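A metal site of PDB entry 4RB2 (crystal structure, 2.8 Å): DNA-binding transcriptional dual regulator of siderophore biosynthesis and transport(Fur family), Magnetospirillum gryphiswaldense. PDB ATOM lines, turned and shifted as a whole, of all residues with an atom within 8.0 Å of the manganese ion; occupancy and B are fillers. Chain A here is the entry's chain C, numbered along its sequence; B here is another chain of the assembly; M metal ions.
Four residues have an atom within 4 Å of the manganese ion: His 89, Asp 91, Glu 110 and His 127. The nearest printed residue that does not touch the manganese ion is Gln 113 (4.1 Å).
A ring nitrogen (NE2) of His 127 lies close to the side-chain amide nitrogen of Gln 113, 3.5 Å away. The backbone NH (N) of Asp 91 sits at hydrogen-bond distance from the backbone carbonyl oxygen (O) of Phe 104, 2.8 Å away.
The manganese ion is bound by a ring nitrogen (NE2) of His 127, the side-chain carboxylate (OD1) of Asp 91, a ring nitrogen (NE2) of His 89, the side-chain carboxylate (OE1) of Glu 110 and the side-chain carboxylate (OE2) of Glu 110. The manganese ion has five donor atoms within binding distance. Slightly farther from the manganese ion lies the side-chain carboxylate (OD2) of Asp 91 (2.8 Å).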
ATOM      1  N   HIS A  89       6.023  -5.718  26.991  1.00  0.00           N
ATOM      2  CA  HIS A  89       5.006  -6.747  26.772  1.00  0.00           C
ATOM      3  C   HIS A  89       4.441  -7.222  28.097  1.00  0.00           C
ATOM      4  O   HIS A  89       5.156  -7.330  29.094  1.00  0.00           O
ATOM      5  CB  HIS A  89       5.567  -7.952  26.014  1.00  0.00           C
ATOM      6  CG  HIS A  89       4.749  -9.197  26.172  1.00  0.00           C
ATOM      7  ND1 HIS A  89       3.566  -9.409  25.496  1.00  0.00           N
ATOM      8  CD2 HIS A  89       4.938 -10.289  26.958  1.00  0.00           C
ATOM      9  CE1 HIS A  89       3.069 -10.576  25.849  1.00  0.00           C
ATOM     10  NE2 HIS A  89       3.879 -11.135  26.732  1.00  0.00           N
ATOM     11  N   HIS A  90       3.145  -7.508  28.101  1.00  0.00           N
ATOM     12  CA  HIS A  90       2.472  -8.058  29.268  1.00  0.00           C
ATOM     13  C   HIS A  90       1.279  -8.880  28.807  1.00  0.00           C
ATOM     14  O   HIS A  90       0.799  -8.734  27.671  1.00  0.00           O
ATOM     15  CB  HIS A  90       2.024  -6.928  30.205  1.00  0.00           C
ATOM     16  CG  HIS A  90       1.064  -5.974  29.569  1.00  0.00           C
ATOM     17  ND1 HIS A  90       1.458  -5.000  28.686  1.00  0.00           N
ATOM     18  CD2 HIS A  90      -0.274  -5.845  29.699  1.00  0.00           C
ATOM     19  CE1 HIS A  90       0.402  -4.307  28.292  1.00  0.00           C
ATOM     20  NE2 HIS A  90      -0.672  -4.807  28.890  1.00  0.00           N
ATOM     21  N   ASP A  91       0.807  -9.745  29.693  1.00  0.00           N
ATOM     22  CA  ASP A  91      -0.421 -10.490  29.432  1.00  0.00           C
ATOM     23  C   ASP A  91      -1.551  -9.864  30.247  1.00  0.00           C
ATOM     24  O   ASP A  91      -1.394  -8.746  30.756  1.00  0.00           O
ATOM     25  CB  ASP A  91      -0.204 -11.967  29.769  1.00  0.00           C
ATOM     26  CG  ASP A  91       1.155 -12.477  29.286  1.00  0.00           C
ATOM     27  OD1 ASP A  91       1.510 -12.202  28.120  1.00  0.00           O
ATOM     28  OD2 ASP A  91       1.864 -13.135  30.067  1.00  0.00           O
ATOM     29  N   HIS A  92      -2.695 -10.538  30.377  1.00  0.00           N
ATOM     30  CA  HIS A  92      -3.818  -9.952  31.108  1.00  0.00           C
ATOM     31  C   HIS A  92      -4.540 -10.918  32.058  1.00  0.00           C
ATOM     32  O   HIS A  92      -4.767 -12.089  31.746  1.00  0.00           O
ATOM     33  CB  HIS A  92      -4.833  -9.290  30.168  1.00  0.00           C
ATOM     34  CG  HIS A  92      -4.218  -8.317  29.226  1.00  0.00           C
ATOM     35  ND1 HIS A  92      -3.679  -8.702  28.016  1.00  0.00           N
ATOM     36  CD2 HIS A  92      -4.026  -6.983  29.318  1.00  0.00           C
ATOM     37  CE1 HIS A  92      -3.189  -7.635  27.392  1.00  0.00           C
ATOM     38  NE2 HIS A  92      -3.388  -6.580  28.165  1.00  0.00           N
ATOM     39  N   PHE A 104       0.144  -8.060  33.805  1.00  0.00           N
ATOM     40  CA  PHE A 104       1.250  -8.817  34.416  1.00  0.00           C
ATOM     41  C   PHE A 104       2.279  -9.392  33.442  1.00  0.00           C
ATOM     42  O   PHE A 104       2.017  -9.604  32.250  1.00  0.00           O
ATOM     43  CB  PHE A 104       0.701  -9.945  35.310  1.00  0.00           C
ATOM     44  CG  PHE A 104       0.282 -11.181  34.547  1.00  0.00           C
ATOM     45  CD1 PHE A 104      -0.985 -11.259  33.975  1.00  0.00           C
ATOM     46  CD2 PHE A 104       1.151 -12.264  34.412  1.00  0.00           C
ATOM     47  CE1 PHE A 104      -1.374 -12.392  33.275  1.00  0.00           C
ATOM     48  CE2 PHE A 104       0.766 -13.388  33.712  1.00  0.00           C
ATOM     49  CZ  PHE A 104      -0.495 -13.458  33.141  1.00  0.00           C
ATOM     50  N   THR A 105       3.462  -9.652  33.996  1.00  0.00           N
ATOM     51  CA  THR A 105       4.563 -10.275  33.283  1.00  0.00           C
ATOM     52  C   THR A 105       5.073 -11.436  34.117  1.00  0.00           C
ATOM     53  O   THR A 105       5.289 -11.281  35.327  1.00  0.00           O
ATOM     54  CB  THR A 105       5.731  -9.280  33.062  1.00  0.00           C
ATOM     55  OG1 THR A 105       5.983  -8.551  34.270  1.00  0.00           O
ATOM     56  CG2 THR A 105       5.432  -8.307  31.933  1.00  0.00           C
ATOM     57  N   SER A 106       5.243 -12.590  33.498  1.00  0.00           N
ATOM     58  CA  SER A 106       5.888 -13.706  34.165  1.00  0.00           C
ATOM     59  C   SER A 106       6.947 -14.233  33.221  1.00  0.00           C
ATOM     60  O   SER A 106       6.628 -14.919  32.256  1.00  0.00           O
ATOM     61  CB  SER A 106       4.898 -14.798  34.522  1.00  0.00           C
ATOM     62  OG  SER A 106       5.555 -15.918  35.081  1.00  0.00           O
ATOM     63  N   PRO A 107       8.227 -13.907  33.509  1.00  0.00           N
ATOM     64  CA  PRO A 107       9.345 -14.293  32.641  1.00  0.00           C
ATOM     65  C   PRO A 107       9.474 -15.813  32.509  1.00  0.00           C
ATOM     66  O   PRO A 107       9.903 -16.306  31.457  1.00  0.00           O
ATOM     67  CB  PRO A 107      10.569 -13.707  33.363  1.00  0.00           C
ATOM     68  CG  PRO A 107      10.016 -12.676  34.301  1.00  0.00           C
ATOM     69  CD  PRO A 107       8.691 -13.219  34.726  1.00  0.00           C
ATOM     70  N   ILE A 109       6.959 -18.033  32.434  1.00  0.00           N
ATOM     71  CA  ILE A 109       5.956 -18.460  31.454  1.00  0.00           C
ATOM     72  C   ILE A 109       6.440 -18.171  30.032  1.00  0.00           C
ATOM     73  O   ILE A 109       6.468 -19.071  29.188  1.00  0.00           O
ATOM     74  CB  ILE A 109       4.589 -17.778  31.689  1.00  0.00           C
ATOM     75  CG1 ILE A 109       4.030 -18.167  33.056  1.00  0.00           C
ATOM     76  CG2 ILE A 109       3.607 -18.163  30.570  1.00  0.00           C
ATOM     77  CD1 ILE A 109       2.640 -17.645  33.340  1.00  0.00           C
ATOM     78  N   GLU A 110       6.840 -16.926  29.812  1.00  0.00           N
ATOM     79  CA  GLU A 110       7.415 -16.488  28.537  1.00  0.00           C
ATOM     80  C   GLU A 110       8.563 -17.412  28.133  1.00  0.00           C
ATOM     81  O   GLU A 110       8.781 -17.645  26.951  1.00  0.00           O
ATOM     82  CB  GLU A 110       7.924 -15.047  28.633  1.00  0.00           C
ATOM     83  CG  GLU A 110       7.024 -14.084  29.412  1.00  0.00           C
ATOM     84  CD  GLU A 110       5.754 -13.684  28.682  1.00  0.00           C
ATOM     85  OE1 GLU A 110       4.804 -13.249  29.371  1.00  0.00           O
ATOM     86  OE2 GLU A 110       5.702 -13.782  27.434  1.00  0.00           O
ATOM     87  N   ALA A 111       9.275 -17.926  29.137  1.00  0.00           N
ATOM     88  CA  ALA A 111      10.411 -18.820  28.907  1.00  0.00           C
ATOM     89  C   ALA A 111       9.970 -20.262  28.685  1.00  0.00           C
ATOM     90  O   ALA A 111      10.573 -20.974  27.882  1.00  0.00           O
ATOM     91  CB  ALA A 111      11.401 -18.731  30.058  1.00  0.00           C
ATOM     92  N   GLN A 113       7.154 -20.938  27.414  1.00  0.00           N
ATOM     93  CA  GLN A 113       6.556 -20.810  26.089  1.00  0.00           C
ATOM     94  C   GLN A 113       7.619 -21.072  25.028  1.00  0.00           C
ATOM     95  O   GLN A 113       7.401 -21.891  24.123  1.00  0.00           O
ATOM     96  CB  GLN A 113       5.943 -19.422  25.885  1.00  0.00           C
ATOM     97  CG  GLN A 113       4.646 -19.184  26.650  1.00  0.00           C
ATOM     98  CD  GLN A 113       4.224 -17.732  26.649  1.00  0.00           C
ATOM     99  OE1 GLN A 113       3.312 -17.329  27.391  1.00  0.00           O
ATOM    100  NE2 GLN A 113       4.880 -16.911  25.837  1.00  0.00           N
ATOM    101  N   GLY A 126       4.989 -15.226  18.339  1.00  0.00           N
ATOM    102  CA  GLY A 126       3.930 -14.497  19.043  1.00  0.00           C
ATOM    103  C   GLY A 126       3.123 -15.405  19.967  1.00  0.00           C
ATOM    104  O   GLY A 126       3.191 -16.638  19.852  1.00  0.00           O
ATOM    105  N   HIS A 127       2.371 -14.794  20.876  1.00  0.00           N
ATOM    106  CA  HIS A 127       1.554 -15.544  21.829  1.00  0.00           C
ATOM    107  C   HIS A 127       0.449 -14.686  22.418  1.00  0.00           C
ATOM    108  O   HIS A 127       0.584 -13.474  22.530  1.00  0.00           O
ATOM    109  CB  HIS A 127       2.420 -16.148  22.945  1.00  0.00           C
ATOM    110  CG  HIS A 127       2.857 -15.153  23.972  1.00  0.00           C
ATOM    111  ND1 HIS A 127       3.887 -14.273  23.758  1.00  0.00           N
ATOM    112  CD2 HIS A 127       2.394 -14.906  25.226  1.00  0.00           C
ATOM    113  CE1 HIS A 127       4.051 -13.516  24.829  1.00  0.00           C
ATOM    114  NE2 HIS A 127       3.165 -13.882  25.736  1.00  0.00           N
ATOM    115  N   ARG A 128      -0.643 -15.347  22.804  1.00  0.00           N
ATOM    116  CA  ARG A 128      -1.724 -14.718  23.547  1.00  0.00           C
ATOM    117  C   ARG A 128      -1.874 -15.422  24.883  1.00  0.00           C
ATOM    118  O   ARG A 128      -1.857 -16.661  24.954  1.00  0.00           O
ATOM    119  CB  ARG A 128      -3.039 -14.797  22.778  1.00  0.00           C
ATOM    120  CG  ARG A 128      -4.073 -13.784  23.229  1.00  0.00           C
ATOM    121  CD  ARG A 128      -5.453 -14.066  22.656  1.00  0.00           C
ATOM    122  NE  ARG A 128      -5.461 -14.443  21.242  1.00  0.00           N
ATOM    123  CZ  ARG A 128      -6.483 -14.269  20.404  1.00  0.00           C
ATOM    124  NH1 ARG A 128      -7.611 -13.695  20.827  1.00  0.00           N
ATOM    125  NH2 ARG A 128      -6.371 -14.649  19.138  1.00  0.00           N
ATOM    126  N   LEU A 129      -2.036 -14.634  25.937  1.00  0.00           N
ATOM    127  CA  LEU A 129      -2.342 -15.200  27.247  1.00  0.00           C
ATOM    128  C   LEU A 129      -3.326 -14.320  27.981  1.00  0.00           C
ATOM    129  O   LEU A 129      -3.184 -13.090  28.018  1.00  0.00           O
ATOM    130  CB  LEU A 129      -1.073 -15.411  28.082  1.00  0.00           C
ATOM    131  CG  LEU A 129      -1.219 -16.076  29.455  1.00  0.00           C
ATOM    132  CD1 LEU A 129      -1.726 -17.506  29.351  1.00  0.00           C
ATOM    133  CD2 LEU A 129       0.123 -16.030  30.168  1.00  0.00           C
ATOM    134  N   GLU A 130      -4.345 -14.967  28.527  1.00  0.00           N
ATOM    135  CA  GLU A 130      -5.373 -14.314  29.293  1.00  0.00           C
ATOM    136  C   GLU A 130      -5.775 -15.245  30.410  1.00  0.00           C
ATOM    137  O   GLU A 130      -6.024 -16.427  30.181  1.00  0.00           O
ATOM    138  CB  GLU A 130      -6.559 -13.980  28.394  1.00  0.00           C
ATOM    139  CG  GLU A 130      -6.349 -12.679  27.632  1.00  0.00           C
ATOM    140  CD  GLU A 130      -6.873 -12.725  26.203  1.00  0.00           C
ATOM    141  OE1 GLU A 130      -6.135 -12.267  25.305  1.00  0.00           O
ATOM    142  OE2 GLU A 130      -8.002 -13.206  25.994  1.00  0.00           O
ATOM    143  N   LEU B 129      -4.470 -19.737  26.365  1.00  0.00           N
ATOM    144  CA  LEU B 129      -3.086 -19.592  25.871  1.00  0.00           C
ATOM    145  C   LEU B 129      -2.917 -20.116  24.439  1.00  0.00           C
ATOM    146  O   LEU B 129      -3.037 -21.318  24.190  1.00  0.00           O
ATOM    147  CB  LEU B 129      -2.059 -20.259  26.792  1.00  0.00           C
ATOM    148  CG  LEU B 129      -0.607 -20.481  26.304  1.00  0.00           C
ATOM    149  CD1 LEU B 129       0.082 -19.186  25.873  1.00  0.00           C
ATOM    150  CD2 LEU B 129       0.235 -21.181  27.360  1.00  0.00           C
ATOM    151  N   GLU B 130      -2.646 -19.191  23.525  1.00  0.00           N
ATOM    152  CA  GLU B 130      -2.264 -19.513  22.159  1.00  0.00           C
ATOM    153  C   GLU B 130      -0.803 -19.223  21.973  1.00  0.00           C
ATOM    154  O   GLU B 130      -0.329 -18.140  22.308  1.00  0.00           O
ATOM    155  CB  GLU B 130      -3.040 -18.660  21.159  1.00  0.00           C
ATOM    156  CG  GLU B 130      -4.246 -19.334  20.556  1.00  0.00           C
ATOM    157  CD  GLU B 130      -5.495 -19.045  21.333  1.00  0.00           C
ATOM    158  OE1 GLU B 130      -5.725 -19.714  22.362  1.00  0.00           O
ATOM    159  OE2 GLU B 130      -6.244 -18.136  20.909  1.00  0.00           O
ATOM    160  N   LEU B 131      -0.078 -20.188  21.403  1.00  0.00           N
ATOM    161  CA  LEU B 131       1.271 -19.930  20.941  1.00  0.00           C
ATOM    162  C   LEU B 131       1.246 -19.841  19.426  1.00  0.00           C
ATOM    163  O   LEU B 131       0.531 -20.594  18.772  1.00  0.00           O
ATOM    164  CB  LEU B 131       2.241 -21.008  21.402  1.00  0.00           C
ATOM    165  CG  LEU B 131       2.567 -21.083  22.892  1.00  0.00           C
ATOM    166  CD1 LEU B 131       3.713 -22.040  23.142  1.00  0.00           C
ATOM    167  CD2 LEU B 131       2.896 -19.710  23.433  1.00  0.00           C
HETATM  168 MN    MN M   1       3.056 -13.284  27.557  1.00  0.00          MN
